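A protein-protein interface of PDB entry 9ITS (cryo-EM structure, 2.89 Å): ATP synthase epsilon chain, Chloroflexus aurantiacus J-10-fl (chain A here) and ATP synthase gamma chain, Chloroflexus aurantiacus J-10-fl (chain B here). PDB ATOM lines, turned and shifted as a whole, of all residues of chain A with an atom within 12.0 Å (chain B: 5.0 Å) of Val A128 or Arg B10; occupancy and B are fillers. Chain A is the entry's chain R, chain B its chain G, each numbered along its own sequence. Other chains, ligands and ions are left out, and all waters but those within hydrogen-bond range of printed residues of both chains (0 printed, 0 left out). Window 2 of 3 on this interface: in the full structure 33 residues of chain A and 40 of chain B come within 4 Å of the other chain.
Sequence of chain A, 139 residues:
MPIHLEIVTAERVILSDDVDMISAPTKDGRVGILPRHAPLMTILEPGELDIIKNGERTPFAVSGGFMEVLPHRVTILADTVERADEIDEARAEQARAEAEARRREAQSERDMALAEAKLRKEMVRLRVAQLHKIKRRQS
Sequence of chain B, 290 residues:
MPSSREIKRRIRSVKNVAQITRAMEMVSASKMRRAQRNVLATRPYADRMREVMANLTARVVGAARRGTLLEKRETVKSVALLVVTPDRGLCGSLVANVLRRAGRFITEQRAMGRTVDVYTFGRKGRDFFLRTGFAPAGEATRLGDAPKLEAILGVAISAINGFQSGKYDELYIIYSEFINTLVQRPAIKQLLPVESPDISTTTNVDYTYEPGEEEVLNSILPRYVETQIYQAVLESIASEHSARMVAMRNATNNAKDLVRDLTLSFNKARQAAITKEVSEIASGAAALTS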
ATOM      1  N   LYS A 118       1.063 -14.970  -7.842  1.00  0.00           N
ATOM      2  CA  LYS A 118       0.518 -13.615  -7.792  1.00  0.00           C
ATOM      3  C   LYS A 118       1.627 -12.579  -7.688  1.00  0.00           C
ATOM      4  O   LYS A 118       1.575 -11.531  -8.340  1.00  0.00           O
ATOM      5  CB  LYS A 118      -0.443 -13.468  -6.612  1.00  0.00           C
ATOM      6  CG  LYS A 118      -1.727 -14.260  -6.731  1.00  0.00           C
ATOM      7  CD  LYS A 118      -2.699 -13.893  -5.620  1.00  0.00           C
ATOM      8  CE  LYS A 118      -2.090 -14.131  -4.249  1.00  0.00           C
ATOM      9  NZ  LYS A 118      -3.036 -13.781  -3.154  1.00  0.00           N
ATOM     10  N   LEU A 119       2.642 -12.859  -6.873  1.00  0.00           N
ATOM     11  CA  LEU A 119       3.717 -11.897  -6.660  1.00  0.00           C
ATOM     12  C   LEU A 119       4.577 -11.735  -7.905  1.00  0.00           C
ATOM     13  O   LEU A 119       4.973 -10.616  -8.244  1.00  0.00           O
ATOM     14  CB  LEU A 119       4.566 -12.322  -5.469  1.00  0.00           C
ATOM     15  CG  LEU A 119       3.815 -12.235  -4.144  1.00  0.00           C
ATOM     16  CD1 LEU A 119       4.217 -13.376  -3.237  1.00  0.00           C
ATOM     17  CD2 LEU A 119       4.075 -10.898  -3.483  1.00  0.00           C
ATOM     18  N   ARG A 120       4.882 -12.837  -8.595  1.00  0.00           N
ATOM     19  CA  ARG A 120       5.609 -12.731  -9.855  1.00  0.00           C
ATOM     20  C   ARG A 120       4.791 -11.974 -10.890  1.00  0.00           C
ATOM     21  O   ARG A 120       5.336 -11.163 -11.647  1.00  0.00           O
ATOM     22  CB  ARG A 120       5.980 -14.117 -10.380  1.00  0.00           C
ATOM     23  CG  ARG A 120       7.135 -14.776  -9.649  1.00  0.00           C
ATOM     24  CD  ARG A 120       7.382 -16.179 -10.174  1.00  0.00           C
ATOM     25  NE  ARG A 120       6.283 -17.086  -9.863  1.00  0.00           N
ATOM     26  CZ  ARG A 120       6.331 -18.401 -10.022  1.00  0.00           C
ATOM     27  NH1 ARG A 120       7.415 -19.003 -10.484  1.00  0.00           N
ATOM     28  NH2 ARG A 120       5.264 -19.131  -9.710  1.00  0.00           N
ATOM     29  N   LYS A 121       3.480 -12.219 -10.928  1.00  0.00           N
ATOM     30  CA  LYS A 121       2.614 -11.499 -11.857  1.00  0.00           C
ATOM     31  C   LYS A 121       2.627 -10.002 -11.572  1.00  0.00           C
ATOM     32  O   LYS A 121       2.736  -9.184 -12.492  1.00  0.00           O
ATOM     33  CB  LYS A 121       1.196 -12.061 -11.772  1.00  0.00           C
ATOM     34  CG  LYS A 121       0.196 -11.365 -12.665  1.00  0.00           C
ATOM     35  CD  LYS A 121      -1.138 -12.089 -12.663  1.00  0.00           C
ATOM     36  CE  LYS A 121      -1.713 -12.187 -11.262  1.00  0.00           C
ATOM     37  NZ  LYS A 121      -1.663 -10.886 -10.546  1.00  0.00           N
ATOM     38  N   GLU A 122       2.540  -9.626 -10.295  1.00  0.00           N
ATOM     39  CA  GLU A 122       2.556  -8.210  -9.940  1.00  0.00           C
ATOM     40  C   GLU A 122       3.916  -7.578 -10.217  1.00  0.00           C
ATOM     41  O   GLU A 122       3.989  -6.429 -10.664  1.00  0.00           O
ATOM     42  CB  GLU A 122       2.168  -8.033  -8.473  1.00  0.00           C
ATOM     43  CG  GLU A 122       0.757  -8.489  -8.155  1.00  0.00           C
ATOM     44  CD  GLU A 122       0.378  -8.261  -6.706  1.00  0.00           C
ATOM     45  OE1 GLU A 122       0.923  -7.325  -6.088  1.00  0.00           O
ATOM     46  OE2 GLU A 122      -0.468  -9.017  -6.185  1.00  0.00           O
ATOM     47  N   MET A 123       5.002  -8.309  -9.953  1.00  0.00           N
ATOM     48  CA  MET A 123       6.336  -7.752 -10.151  1.00  0.00           C
ATOM     49  C   MET A 123       6.645  -7.553 -11.629  1.00  0.00           C
ATOM     50  O   MET A 123       7.157  -6.499 -12.022  1.00  0.00           O
ATOM     51  CB  MET A 123       7.385  -8.652  -9.500  1.00  0.00           C
ATOM     52  CG  MET A 123       7.469  -8.508  -7.990  1.00  0.00           C
ATOM     53  SD  MET A 123       7.983  -6.858  -7.474  1.00  0.00           S
ATOM     54  CE  MET A 123       9.701  -6.862  -7.979  1.00  0.00           C
ATOM     55  N   VAL A 124       6.341  -8.549 -12.469  1.00  0.00           N
ATOM     56  CA  VAL A 124       6.521  -8.376 -13.910  1.00  0.00           C
ATOM     57  C   VAL A 124       5.391  -7.578 -14.533  1.00  0.00           C
ATOM     58  O   VAL A 124       5.412  -7.328 -15.744  1.00  0.00           O
ATOM     59  CB  VAL A 124       6.646  -9.727 -14.640  1.00  0.00           C
ATOM     60  CG1 VAL A 124       7.665 -10.616 -13.944  1.00  0.00           C
ATOM     61  CG2 VAL A 124       5.297 -10.415 -14.735  1.00  0.00           C
ATOM     62  N   ARG A 125       4.406  -7.168 -13.734  1.00  0.00           N
ATOM     63  CA  ARG A 125       3.287  -6.399 -14.261  1.00  0.00           C
ATOM     64  C   ARG A 125       3.602  -4.911 -14.316  1.00  0.00           C
ATOM     65  O   ARG A 125       3.389  -4.259 -15.343  1.00  0.00           O
ATOM     66  CB  ARG A 125       2.052  -6.645 -13.404  1.00  0.00           C
ATOM     67  CG  ARG A 125       0.957  -5.657 -13.668  1.00  0.00           C
ATOM     68  CD  ARG A 125       0.317  -5.913 -15.014  1.00  0.00           C
ATOM     69  NE  ARG A 125       0.094  -7.334 -15.241  1.00  0.00           N
ATOM     70  CZ  ARG A 125      -0.832  -8.055 -14.625  1.00  0.00           C
ATOM     71  NH1 ARG A 125      -1.628  -7.523 -13.715  1.00  0.00           N
ATOM     72  NH2 ARG A 125      -0.966  -9.339 -14.935  1.00  0.00           N
ATOM     73  N   LEU A 126       4.091  -4.349 -13.216  1.00  0.00           N
ATOM     74  CA  LEU A 126       4.331  -2.917 -13.137  1.00  0.00           C
ATOM     75  C   LEU A 126       5.639  -2.500 -13.792  1.00  0.00           C
ATOM     76  O   LEU A 126       5.914  -1.300 -13.886  1.00  0.00           O
ATOM     77  CB  LEU A 126       4.294  -2.454 -11.681  1.00  0.00           C
ATOM     78  CG  LEU A 126       2.860  -2.196 -11.216  1.00  0.00           C
ATOM     79  CD1 LEU A 126       2.799  -1.890  -9.731  1.00  0.00           C
ATOM     80  CD2 LEU A 126       2.245  -1.069 -12.033  1.00  0.00           C
ATOM     81  N   ARG A 127       6.424  -3.482 -14.244  1.00  0.00           N
ATOM     82  CA  ARG A 127       7.686  -3.170 -14.966  1.00  0.00           C
ATOM     83  C   ARG A 127       7.355  -2.968 -16.447  1.00  0.00           C
ATOM     84  O   ARG A 127       8.131  -2.277 -17.136  1.00  0.00           O
ATOM     85  CB  ARG A 127       8.706  -4.297 -14.777  1.00  0.00           C
ATOM     86  CG  ARG A 127       8.287  -5.623 -15.396  1.00  0.00           C
ATOM     87  CD  ARG A 127       9.368  -6.678 -15.260  1.00  0.00           C
ATOM     88  NE  ARG A 127       9.027  -7.904 -15.967  1.00  0.00           N
ATOM     89  CZ  ARG A 127       9.817  -8.967 -16.060  1.00  0.00           C
ATOM     90  NH1 ARG A 127      11.007  -8.959 -15.482  1.00  0.00           N
ATOM     91  NH2 ARG A 127       9.416 -10.032 -16.729  1.00  0.00           N
ATOM     92  N   VAL A 128       6.237  -3.540 -16.907  1.00  0.00           N
ATOM     93  CA  VAL A 128       5.813  -3.382 -18.330  1.00  0.00           C
ATOM     94  C   VAL A 128       5.625  -1.891 -18.614  1.00  0.00           C
ATOM     95  O   VAL A 128       5.928  -1.465 -19.746  1.00  0.00           O
ATOM     96  CB  VAL A 128       4.518  -4.162 -18.624  1.00  0.00           C
ATOM     97  CG1 VAL A 128       4.113  -4.054 -20.086  1.00  0.00           C
ATOM     98  CG2 VAL A 128       4.623  -5.619 -18.203  1.00  0.00           C
ATOM     99  N   ALA A 129       5.134  -1.135 -17.624  1.00  0.00           N
ATOM    100  CA  ALA A 129       4.861   0.305 -17.834  1.00  0.00           C
ATOM    101  C   ALA A 129       3.877   0.448 -18.998  1.00  0.00           C
ATOM    102  O   ALA A 129       2.739  -0.047 -18.870  1.00  0.00           O
ATOM    103  CB  ALA A 129       6.148   1.047 -18.095  1.00  0.00           C
ATOM    104  N   GLN A 130       4.302   1.089 -20.090  1.00  0.00           N
ATOM    105  CA  GLN A 130       3.427   1.201 -21.286  1.00  0.00           C
ATOM    106  C   GLN A 130       2.969  -0.206 -21.687  1.00  0.00           C
ATOM    107  O   GLN A 130       3.837  -1.092 -21.812  1.00  0.00           O
ATOM    108  CB  GLN A 130       4.172   1.887 -22.431  1.00  0.00           C
ATOM    109  CG  GLN A 130       3.375   1.949 -23.726  1.00  0.00           C
ATOM    110  CD  GLN A 130       4.139   2.635 -24.831  1.00  0.00           C
ATOM    111  OE1 GLN A 130       5.254   3.115 -24.637  1.00  0.00           O
ATOM    112  NE2 GLN A 130       3.541   2.685 -26.010  1.00  0.00           N
ATOM    113  N   LEU A 131       1.660  -0.397 -21.869  1.00  0.00           N
ATOM    114  CA  LEU A 131       1.112  -1.735 -22.222  1.00  0.00           C
ATOM    115  C   LEU A 131       1.997  -2.376 -23.296  1.00  0.00           C
ATOM    116  O   LEU A 131       2.149  -1.791 -24.368  1.00  0.00           O
ATOM    117  CB  LEU A 131      -0.328  -1.571 -22.719  1.00  0.00           C
ATOM    118  CG  LEU A 131      -1.368  -1.229 -21.651  1.00  0.00           C
ATOM    119  CD1 LEU A 131      -1.124   0.156 -21.070  1.00  0.00           C
ATOM    120  CD2 LEU A 131      -2.775  -1.319 -22.221  1.00  0.00           C
ATOM    121  N   PRO B   2       9.503   3.601 -28.639  1.00  0.00           N
ATOM    122  CA  PRO B   2      10.312   3.800 -27.431  1.00  0.00           C
ATOM    123  C   PRO B   2      11.730   3.285 -27.620  1.00  0.00           C
ATOM    124  O   PRO B   2      12.695   4.053 -27.554  1.00  0.00           O
ATOM    125  CB  PRO B   2       9.558   2.996 -26.364  1.00  0.00           C
ATOM    126  CG  PRO B   2       8.168   2.866 -26.888  1.00  0.00           C
ATOM    127  CD  PRO B   2       8.297   2.799 -28.377  1.00  0.00           C
ATOM    128  N   GLU B   6      13.259  -1.970 -25.095  1.00  0.00           N
ATOM    129  CA  GLU B   6      12.184  -1.752 -24.132  1.00  0.00           C
ATOM    130  C   GLU B   6      10.919  -2.504 -24.525  1.00  0.00           C
ATOM    131  O   GLU B   6      10.261  -3.112 -23.672  1.00  0.00           O
ATOM    132  CB  GLU B   6      11.906  -0.258 -23.993  1.00  0.00           C
ATOM    133  CG  GLU B   6      13.098   0.536 -23.484  1.00  0.00           C
ATOM    134  CD  GLU B   6      12.956   2.024 -23.725  1.00  0.00           C
ATOM    135  OE1 GLU B   6      11.872   2.454 -24.165  1.00  0.00           O
ATOM    136  OE2 GLU B   6      13.931   2.763 -23.474  1.00  0.00           O
ATOM    137  N   ILE B   7      10.563  -2.482 -25.811  1.00  0.00           N
ATOM    138  CA  ILE B   7       9.393  -3.233 -26.251  1.00  0.00           C
ATOM    139  C   ILE B   7       9.635  -4.731 -26.128  1.00  0.00           C
ATOM    140  O   ILE B   7       8.712  -5.486 -25.810  1.00  0.00           O
ATOM    141  CB  ILE B   7       8.990  -2.833 -27.682  1.00  0.00           C
ATOM    142  CG1 ILE B   7       8.733  -1.331 -27.761  1.00  0.00           C
ATOM    143  CG2 ILE B   7       7.724  -3.550 -28.096  1.00  0.00           C
ATOM    144  CD1 ILE B   7       8.563  -0.825 -29.171  1.00  0.00           C
ATOM    145  N   LYS B   8      10.866  -5.193 -26.362  1.00  0.00           N
ATOM    146  CA  LYS B   8      11.167  -6.608 -26.160  1.00  0.00           C
ATOM    147  C   LYS B   8      11.025  -7.000 -24.693  1.00  0.00           C
ATOM    148  O   LYS B   8      10.511  -8.080 -24.375  1.00  0.00           O
ATOM    149  CB  LYS B   8      12.573  -6.925 -26.667  1.00  0.00           C
ATOM    150  CG  LYS B   8      12.891  -8.407 -26.714  1.00  0.00           C
ATOM    151  CD  LYS B   8      14.357  -8.647 -27.029  1.00  0.00           C
ATOM    152  CE  LYS B   8      14.635  -8.496 -28.514  1.00  0.00           C
ATOM    153  NZ  LYS B   8      16.036  -8.873 -28.855  1.00  0.00           N
ATOM    154  N   ARG B   9      11.478  -6.133 -23.785  1.00  0.00           N
ATOM    155  CA  ARG B   9      11.304  -6.391 -22.359  1.00  0.00           C
ATOM    156  C   ARG B   9       9.829  -6.427 -21.982  1.00  0.00           C
ATOM    157  O   ARG B   9       9.402  -7.273 -21.185  1.00  0.00           O
ATOM    158  CB  ARG B   9      12.042  -5.331 -21.543  1.00  0.00           C
ATOM    159  CG  ARG B   9      12.077  -5.607 -20.052  1.00  0.00           C
ATOM    160  CD  ARG B   9      12.606  -4.407 -19.285  1.00  0.00           C
ATOM    161  NE  ARG B   9      12.012  -3.159 -19.749  1.00  0.00           N
ATOM    162  CZ  ARG B   9      10.836  -2.696 -19.348  1.00  0.00           C
ATOM    163  NH1 ARG B   9      10.097  -3.353 -18.470  1.00  0.00           N
ATOM    164  NH2 ARG B   9      10.391  -1.543 -19.841  1.00  0.00           N
ATOM    165  N   ARG B  10       9.033  -5.515 -22.545  1.00  0.00           N
ATOM    166  CA  ARG B  10       7.594  -5.537 -22.298  1.00  0.00           C
ATOM    167  C   ARG B  10       6.962  -6.817 -22.833  1.00  0.00           C
ATOM    168  O   ARG B  10       6.066  -7.384 -22.200  1.00  0.00           O
ATOM    169  CB  ARG B  10       6.925  -4.316 -22.924  1.00  0.00           C
ATOM    170  CG  ARG B  10       7.280  -2.998 -22.267  1.00  0.00           C
ATOM    171  CD  ARG B  10       6.694  -1.839 -23.050  1.00  0.00           C
ATOM    172  NE  ARG B  10       7.245  -0.556 -22.635  1.00  0.00           N
ATOM    173  CZ  ARG B  10       7.097   0.574 -23.311  1.00  0.00           C
ATOM    174  NH1 ARG B  10       6.416   0.617 -24.444  1.00  0.00           N
ATOM    175  NH2 ARG B  10       7.646   1.690 -22.840  1.00  0.00           N
ATOM    176  N   ILE B  11       7.409  -7.277 -24.003  1.00  0.00           N
ATOM    177  CA  ILE B  11       6.902  -8.524 -24.568  1.00  0.00           C
ATOM    178  C   ILE B  11       7.209  -9.687 -23.638  1.00  0.00           C
ATOM    179  O   ILE B  11       6.352 -10.540 -23.384  1.00  0.00           O
ATOM    180  CB  ILE B  11       7.492  -8.758 -25.971  1.00  0.00           C
ATOM    181  CG1 ILE B  11       6.838  -7.832 -26.990  1.00  0.00           C
ATOM    182  CG2 ILE B  11       7.314 -10.203 -26.401  1.00  0.00           C
ATOM    183  CD1 ILE B  11       7.621  -7.692 -28.264  1.00  0.00           C
ATOM    184  N   ARG B  12       8.434  -9.733 -23.111  1.00  0.00           N
ATOM    185  CA  ARG B  12       8.796 -10.798 -22.180  1.00  0.00           C
ATOM    186  C   ARG B  12       7.949 -10.737 -20.914  1.00  0.00           C
ATOM    187  O   ARG B  12       7.500 -11.772 -20.406  1.00  0.00           O
ATOM    188  CB  ARG B  12      10.283 -10.715 -21.840  1.00  0.00           C
ATOM    189  CG  ARG B  12      10.772 -11.865 -20.983  1.00  0.00           C
ATOM    190  CD  ARG B  12      10.417 -13.196 -21.620  1.00  0.00           C
ATOM    191  NE  ARG B  12      10.808 -14.328 -20.791  1.00  0.00           N
ATOM    192  CZ  ARG B  12      10.301 -15.548 -20.907  1.00  0.00           C
ATOM    193  NH1 ARG B  12       9.376 -15.828 -21.809  1.00  0.00           N
ATOM    194  NH2 ARG B  12      10.733 -16.510 -20.095  1.00  0.00           N
ATOM    195  N   SER B  13       7.711  -9.529 -20.397  1.00  0.00           N
ATOM    196  CA  SER B  13       6.904  -9.383 -19.188  1.00  0.00           C
ATOM    197  C   SER B  13       5.468  -9.843 -19.418  1.00  0.00           C
ATOM    198  O   SER B  13       4.891 -10.553 -18.585  1.00  0.00           O
ATOM    199  CB  SER B  13       6.935  -7.933 -18.710  1.00  0.00           C
ATOM    200  OG  SER B  13       8.241  -7.555 -18.314  1.00  0.00           O
ATOM    201  N   VAL B  14       4.872  -9.454 -20.547  1.00  0.00           N
ATOM    202  CA  VAL B  14       3.493  -9.852 -20.812  1.00  0.00           C
ATOM    203  C   VAL B  14       3.405 -11.343 -21.121  1.00  0.00           C
ATOM    204  O   VAL B  14       2.403 -11.989 -20.798  1.00  0.00           O
ATOM    205  CB  VAL B  14       2.885  -8.989 -21.935  1.00  0.00           C
ATOM    206  CG1 VAL B  14       1.425  -9.337 -22.143  1.00  0.00           C
ATOM    207  CG2 VAL B  14       2.994  -7.524 -21.577  1.00  0.00           C
ATOM    208  N   LYS B  15       4.442 -11.925 -21.728  1.00  0.00           N
ATOM    209  CA  LYS B  15       4.458 -13.373 -21.923  1.00  0.00           C
ATOM    210  C   LYS B  15       4.526 -14.108 -20.589  1.00  0.00           C
ATOM    211  O   LYS B  15       3.854 -15.131 -20.401  1.00  0.00           O
ATOM    212  CB  LYS B  15       5.629 -13.770 -22.817  1.00  0.00           C
ATOM    213  CG  LYS B  15       5.339 -13.652 -24.300  1.00  0.00           C
ATOM    214  CD  LYS B  15       6.542 -14.058 -25.132  1.00  0.00           C
ATOM    215  CE  LYS B  15       6.178 -14.170 -26.601  1.00  0.00           C
ATOM    216  NZ  LYS B  15       7.384 -14.173 -27.470  1.00  0.00           N
ATOM    217  N   LEU B 262       2.177  -5.722 -28.987  1.00  0.00           N
ATOM    218  CA  LEU B 262       3.554  -5.375 -28.672  1.00  0.00           C
ATOM    219  C   LEU B 262       4.527  -5.960 -29.683  1.00  0.00           C
ATOM    220  O   LEU B 262       5.562  -5.354 -29.956  1.00  0.00           O
ATOM    221  CB  LEU B 262       3.905  -5.856 -27.269  1.00  0.00           C
ATOM    222  CG  LEU B 262       3.503  -4.987 -26.082  1.00  0.00           C
ATOM    223  CD1 LEU B 262       3.580  -5.815 -24.819  1.00  0.00           C
ATOM    224  CD2 LEU B 262       4.402  -3.774 -25.986  1.00  0.00           C
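The guanidinium group of Arg A127 is in hydrogen-bond range of the side-chain hydroxyl of Ser B13. NH1 of Arg B10 lies within hydrogen-bond range of OE1 of Gln A130, 2.8 Å away. NE of Arg B10 lies close to O of Val A128 (3.3 Å). The backbone carbonyl oxygen (O) of Arg A127 lies within hydrogen-bond range of the guanidinium group (NH1) of Arg B9 (2.6 Å).
Val A124 touches Ser B13 (O to CB, 3.4 Å). CB of Ser B13 touches CG2 of Val A128, 3.3 Å away. Val A128 touches Val B14. CG of Pro B2 touches OE1 of Gln A130 (3.7 Å). Leu A131 touches Leu B262.
Among the printed residues, 9 pairs touch across the chains.
Val A128 touches just these residues of chain B: Arg B10 (3.2 Å), Ser B13 (3.3 Å) and Val B14 (3.9 Å). Arg B10 touches just these residues of chain A: Val A128 and Gln A130. Of chain A, only Gln A130 (3.7 Å) comes within 4 Å of Pro B2. No residue of chain A comes within 4 Å of Glu B6. No residue of chain A comes within 4 Å of Ile B7. Of chain A, only Arg A127 comes within 4 Å of Arg B9. Of the printed residues of chain A, Val B14 touches Val A128 (3.9 Å). Leu B262 touches just one residue of chain A: Leu A131. Of the printed residues of chain B, Leu A131 touches Leu B262 (3.4 Å). Of the printed residues of chain B, Arg A127 touches Arg B9 (2.6 Å) and Ser B13 (2.5 Å). Printed residues of chain B within 4 Å of Val A124: Ser B13. Of the printed residues of chain B, Gln A130 touches Pro B2 (3.7 Å) and Arg B10 (2.8 Å). Lys B15 touches none of the printed residues of chain A.
OG of Ser B13 is in hydrogen-bond range of O of Arg B9 (3.1 Å).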
